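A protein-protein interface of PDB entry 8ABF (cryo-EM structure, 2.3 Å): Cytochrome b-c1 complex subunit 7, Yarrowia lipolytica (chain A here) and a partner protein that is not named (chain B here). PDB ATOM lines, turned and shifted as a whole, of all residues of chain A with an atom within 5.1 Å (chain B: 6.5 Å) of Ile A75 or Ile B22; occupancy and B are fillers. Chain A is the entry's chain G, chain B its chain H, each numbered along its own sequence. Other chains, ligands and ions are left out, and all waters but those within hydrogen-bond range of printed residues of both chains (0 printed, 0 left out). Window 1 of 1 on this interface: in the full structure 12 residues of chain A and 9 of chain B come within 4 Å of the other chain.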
ATOM      1  N   ARG A  70     -13.242   4.228 -10.543  1.00  0.00           N
ATOM      2  CA  ARG A  70     -12.953   4.632 -11.905  1.00  0.00           C
ATOM      3  C   ARG A  70     -14.243   4.563 -12.722  1.00  0.00           C
ATOM      4  O   ARG A  70     -14.561   5.493 -13.461  1.00  0.00           O
ATOM      5  CB  ARG A  70     -11.835   3.753 -12.465  1.00  0.00           C
ATOM      6  CG  ARG A  70     -11.611   3.917 -13.962  1.00  0.00           C
ATOM      7  CD  ARG A  70     -10.447   3.091 -14.480  1.00  0.00           C
ATOM      8  NE  ARG A  70     -10.305   3.205 -15.928  1.00  0.00           N
ATOM      9  CZ  ARG A  70     -10.991   2.491 -16.820  1.00  0.00           C
ATOM     10  NH1 ARG A  70     -10.765   2.650 -18.117  1.00  0.00           N
ATOM     11  NH2 ARG A  70     -11.854   1.574 -16.410  1.00  0.00           N
ATOM     12  N   VAL A  71     -15.013   3.485 -12.553  1.00  0.00           N
ATOM     13  CA  VAL A  71     -16.265   3.362 -13.283  1.00  0.00           C
ATOM     14  C   VAL A  71     -17.153   4.562 -12.972  1.00  0.00           C
ATOM     15  O   VAL A  71     -17.751   5.157 -13.863  1.00  0.00           O
ATOM     16  CB  VAL A  71     -16.998   2.061 -12.933  1.00  0.00           C
ATOM     17  CG1 VAL A  71     -18.464   2.114 -13.337  1.00  0.00           C
ATOM     18  CG2 VAL A  71     -16.304   0.862 -13.545  1.00  0.00           C
ATOM     19  N   TYR A  72     -17.201   4.976 -11.713  1.00  0.00           N
ATOM     20  CA  TYR A  72     -18.056   6.108 -11.427  1.00  0.00           C
ATOM     21  C   TYR A  72     -17.551   7.396 -12.077  1.00  0.00           C
ATOM     22  O   TYR A  72     -18.338   8.161 -12.615  1.00  0.00           O
ATOM     23  CB  TYR A  72     -18.183   6.311  -9.928  1.00  0.00           C
ATOM     24  CG  TYR A  72     -18.970   7.549  -9.622  1.00  0.00           C
ATOM     25  CD1 TYR A  72     -20.301   7.646 -10.002  1.00  0.00           C
ATOM     26  CD2 TYR A  72     -18.378   8.625  -8.990  1.00  0.00           C
ATOM     27  CE1 TYR A  72     -21.040   8.786  -9.742  1.00  0.00           C
ATOM     28  CE2 TYR A  72     -19.114   9.761  -8.690  1.00  0.00           C
ATOM     29  CZ  TYR A  72     -20.445   9.840  -9.070  1.00  0.00           C
ATOM     30  OH  TYR A  72     -21.185  10.952  -8.804  1.00  0.00           O
ATOM     31  N   ARG A  73     -16.246   7.653 -12.040  1.00  0.00           N
ATOM     32  CA  ARG A  73     -15.751   8.859 -12.685  1.00  0.00           C
ATOM     33  C   ARG A  73     -16.027   8.830 -14.191  1.00  0.00           C
ATOM     34  O   ARG A  73     -16.331   9.848 -14.774  1.00  0.00           O
ATOM     35  CB  ARG A  73     -14.263   9.061 -12.412  1.00  0.00           C
ATOM     36  CG  ARG A  73     -13.913   9.450 -10.981  1.00  0.00           C
ATOM     37  CD  ARG A  73     -12.448   9.879 -10.859  1.00  0.00           C
ATOM     38  NE  ARG A  73     -11.521   8.887 -11.405  1.00  0.00           N
ATOM     39  CZ  ARG A  73     -11.072   7.798 -10.779  1.00  0.00           C
ATOM     40  NH1 ARG A  73     -10.276   6.963 -11.425  1.00  0.00           N
ATOM     41  NH2 ARG A  73     -11.416   7.541  -9.528  1.00  0.00           N
ATOM     42  N   LEU A  74     -15.927   7.682 -14.849  1.00  0.00           N
ATOM     43  CA  LEU A  74     -16.213   7.650 -16.274  1.00  0.00           C
ATOM     44  C   LEU A  74     -17.687   7.939 -16.552  1.00  0.00           C
ATOM     45  O   LEU A  74     -17.994   8.668 -17.491  1.00  0.00           O
ATOM     46  CB  LEU A  74     -15.823   6.282 -16.820  1.00  0.00           C
ATOM     47  CG  LEU A  74     -14.334   5.939 -16.768  1.00  0.00           C
ATOM     48  CD1 LEU A  74     -14.089   4.576 -17.395  1.00  0.00           C
ATOM     49  CD2 LEU A  74     -13.483   7.010 -17.448  1.00  0.00           C
ATOM     50  N   ILE A  75     -18.584   7.367 -15.747  1.00  0.00           N
ATOM     51  CA  ILE A  75     -20.003   7.591 -15.939  1.00  0.00           C
ATOM     52  C   ILE A  75     -20.323   9.046 -15.636  1.00  0.00           C
ATOM     53  O   ILE A  75     -21.017   9.692 -16.393  1.00  0.00           O
ATOM     54  CB  ILE A  75     -20.830   6.629 -15.078  1.00  0.00           C
ATOM     55  CG1 ILE A  75     -20.741   5.222 -15.668  1.00  0.00           C
ATOM     56  CG2 ILE A  75     -22.258   7.124 -14.937  1.00  0.00           C
ATOM     57  CD1 ILE A  75     -21.253   4.113 -14.761  1.00  0.00           C
ATOM     58  N   ARG A  76     -19.823   9.562 -14.526  1.00  0.00           N
ATOM     59  CA  ARG A  76     -20.067  10.949 -14.204  1.00  0.00           C
ATOM     60  C   ARG A  76     -19.561  11.901 -15.303  1.00  0.00           C
ATOM     61  O   ARG A  76     -20.254  12.852 -15.640  1.00  0.00           O
ATOM     62  CB  ARG A  76     -19.392  11.195 -12.864  1.00  0.00           C
ATOM     63  CG  ARG A  76     -19.671  12.565 -12.283  1.00  0.00           C
ATOM     64  CD  ARG A  76     -18.390  13.190 -11.761  1.00  0.00           C
ATOM     65  NE  ARG A  76     -17.938  12.876 -10.471  1.00  0.00           N
ATOM     66  CZ  ARG A  76     -16.746  12.941  -9.938  1.00  0.00           C
ATOM     67  NH1 ARG A  76     -16.784  12.979  -8.627  1.00  0.00           N
ATOM     68  NH2 ARG A  76     -15.621  12.749 -10.609  1.00  0.00           N
ATOM     69  N   ALA A  77     -18.372  11.665 -15.878  1.00  0.00           N
ATOM     70  CA  ALA A  77     -17.801  12.557 -16.883  1.00  0.00           C
ATOM     71  C   ALA A  77     -18.636  12.450 -18.148  1.00  0.00           C
ATOM     72  O   ALA A  77     -18.841  13.446 -18.817  1.00  0.00           O
ATOM     73  CB  ALA A  77     -16.385  12.167 -17.229  1.00  0.00           C
ATOM     74  N   THR A  78     -19.075  11.234 -18.485  1.00  0.00           N
ATOM     75  CA  THR A  78     -19.939  11.059 -19.632  1.00  0.00           C
ATOM     76  C   THR A  78     -21.230  11.859 -19.460  1.00  0.00           C
ATOM     77  O   THR A  78     -21.749  12.405 -20.420  1.00  0.00           O
ATOM     78  CB  THR A  78     -20.256   9.574 -19.819  1.00  0.00           C
ATOM     79  OG1 THR A  78     -18.997   8.915 -19.937  1.00  0.00           O
ATOM     80  CG2 THR A  78     -21.141   9.303 -21.012  1.00  0.00           C
ATOM     81  N   GLN A  79     -21.801  11.879 -18.257  1.00  0.00           N
ATOM     82  CA  GLN A  79     -23.018  12.648 -18.041  1.00  0.00           C
ATOM     83  C   GLN A  79     -22.745  14.151 -18.140  1.00  0.00           C
ATOM     84  O   GLN A  79     -23.564  14.858 -18.702  1.00  0.00           O
ATOM     85  CB  GLN A  79     -23.665  12.255 -16.719  1.00  0.00           C
ATOM     86  CG  GLN A  79     -24.954  13.011 -16.423  1.00  0.00           C
ATOM     87  CD  GLN A  79     -26.104  12.548 -17.284  1.00  0.00           C
ATOM     88  OE1 GLN A  79     -26.183  11.383 -17.666  1.00  0.00           O
ATOM     89  NE2 GLN A  79     -27.024  13.452 -17.587  1.00  0.00           N
ATOM     90  N   SER B  16     -18.006  -3.703 -19.622  1.00  0.00           N
ATOM     91  CA  SER B  16     -17.734  -2.776 -18.533  1.00  0.00           C
ATOM     92  C   SER B  16     -16.992  -3.524 -17.428  1.00  0.00           C
ATOM     93  O   SER B  16     -17.276  -4.688 -17.185  1.00  0.00           O
ATOM     94  CB  SER B  16     -19.027  -2.193 -17.999  1.00  0.00           C
ATOM     95  OG  SER B  16     -18.824  -1.439 -16.810  1.00  0.00           O
ATOM     96  N   GLN B  19     -19.797  -2.940 -12.116  1.00  0.00           N
ATOM     97  CA  GLN B  19     -20.276  -1.702 -11.541  1.00  0.00           C
ATOM     98  C   GLN B  19     -20.964  -2.040 -10.232  1.00  0.00           C
ATOM     99  O   GLN B  19     -21.697  -3.020 -10.152  1.00  0.00           O
ATOM    100  CB  GLN B  19     -21.227  -0.992 -12.495  1.00  0.00           C
ATOM    101  CG  GLN B  19     -20.659  -0.838 -13.893  1.00  0.00           C
ATOM    102  CD  GLN B  19     -21.491   0.100 -14.730  1.00  0.00           C
ATOM    103  OE1 GLN B  19     -22.466   0.689 -14.263  1.00  0.00           O
ATOM    104  NE2 GLN B  19     -21.106   0.253 -15.987  1.00  0.00           N
ATOM    105  N   LYS B  20     -20.699  -1.228  -9.214  1.00  0.00           N
ATOM    106  CA  LYS B  20     -21.362  -1.379  -7.941  1.00  0.00           C
ATOM    107  C   LYS B  20     -21.355  -0.032  -7.235  1.00  0.00           C
ATOM    108  O   LYS B  20     -20.399   0.718  -7.362  1.00  0.00           O
ATOM    109  CB  LYS B  20     -20.578  -2.370  -7.091  1.00  0.00           C
ATOM    110  CG  LYS B  20     -21.337  -2.838  -5.870  1.00  0.00           C
ATOM    111  CD  LYS B  20     -20.697  -4.044  -5.258  1.00  0.00           C
ATOM    112  CE  LYS B  20     -21.231  -4.354  -3.878  1.00  0.00           C
ATOM    113  NZ  LYS B  20     -20.429  -5.413  -3.220  1.00  0.00           N
ATOM    114  N   GLY B  21     -22.424   0.269  -6.496  1.00  0.00           N
ATOM    115  CA  GLY B  21     -22.422   1.440  -5.641  1.00  0.00           C
ATOM    116  C   GLY B  21     -22.985   2.697  -6.302  1.00  0.00           C
ATOM    117  O   GLY B  21     -23.106   3.713  -5.624  1.00  0.00           O
ATOM    118  N   ILE B  22     -23.374   2.639  -7.579  1.00  0.00           N
ATOM    119  CA  ILE B  22     -23.944   3.824  -8.209  1.00  0.00           C
ATOM    120  C   ILE B  22     -25.455   3.688  -8.264  1.00  0.00           C
ATOM    121  O   ILE B  22     -25.956   2.726  -8.823  1.00  0.00           O
ATOM    122  CB  ILE B  22     -23.381   4.026  -9.625  1.00  0.00           C
ATOM    123  CG1 ILE B  22     -21.851   4.049  -9.601  1.00  0.00           C
ATOM    124  CG2 ILE B  22     -23.975   5.270 -10.283  1.00  0.00           C
ATOM    125  CD1 ILE B  22     -21.210   3.855 -10.963  1.00  0.00           C
ATOM    126  N   ALA B  23     -26.184   4.669  -7.731  1.00  0.00           N
ATOM    127  CA  ALA B  23     -27.617   4.670  -7.925  1.00  0.00           C
ATOM    128  C   ALA B  23     -27.906   5.729  -8.976  1.00  0.00           C
ATOM    129  O   ALA B  23     -27.408   6.836  -8.836  1.00  0.00           O
ATOM    130  CB  ALA B  23     -28.277   4.969  -6.606  1.00  0.00           C
ATOM    131  N   GLY B  24     -28.680   5.389 -10.016  1.00  0.00           N
ATOM    132  CA  GLY B  24     -29.048   6.345 -11.047  1.00  0.00           C
ATOM    133  C   GLY B  24     -30.544   6.634 -10.982  1.00  0.00           C
ATOM    134  O   GLY B  24     -31.332   5.741 -10.701  1.00  0.00           O
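The side-chain hydroxyl of Ser B16 sits at hydrogen-bond distance from the side-chain amide nitrogen of Gln B19 (3.0 Å).
Among the printed residues, pairs that only touch across the chains: Ile A75 with Gln B19, Val A71 with Gln B19, Ile A75 with Ile B22 and Tyr A72 with Ile B22.
Arg A70 touches none of the printed residues of chain B.
Of the printed residues of chain B, Val A71 touches Gln B19.
Of the printed residues of chain B, Tyr A72 touches Ile B22 (3.9 Å).
Of chain B, only Gln B19 and Ile B22 come within 4 Å of Ile A75.
Arg A76 touches none of the printed residues of chain B.
Of the printed residues of chain A, Gln B19 touches Val A71 and Ile A75.
Ile B22 touches two residues of chain A.
The nearest residue of chain B that does not touch Ile A75 is Ser B16 (6.4 Å).
Of the 10 printed residues of chain A, 3 touch a printed residue of chain B.
Printed residues of chain A that touch a printed residue of chain B: Val A71, Tyr A72 and Ile A75.
Hydrophobic or aromatic side chains of chain A that line the printed part of chain B: Val A71, Tyr A72 and Ile A75.
Of the 7 printed residues of chain B, 2 touch a printed residue of chain A.
Hydrophobic or aromatic side chains of chain B within 4 Å of the printed part of chain A: Ile B22.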
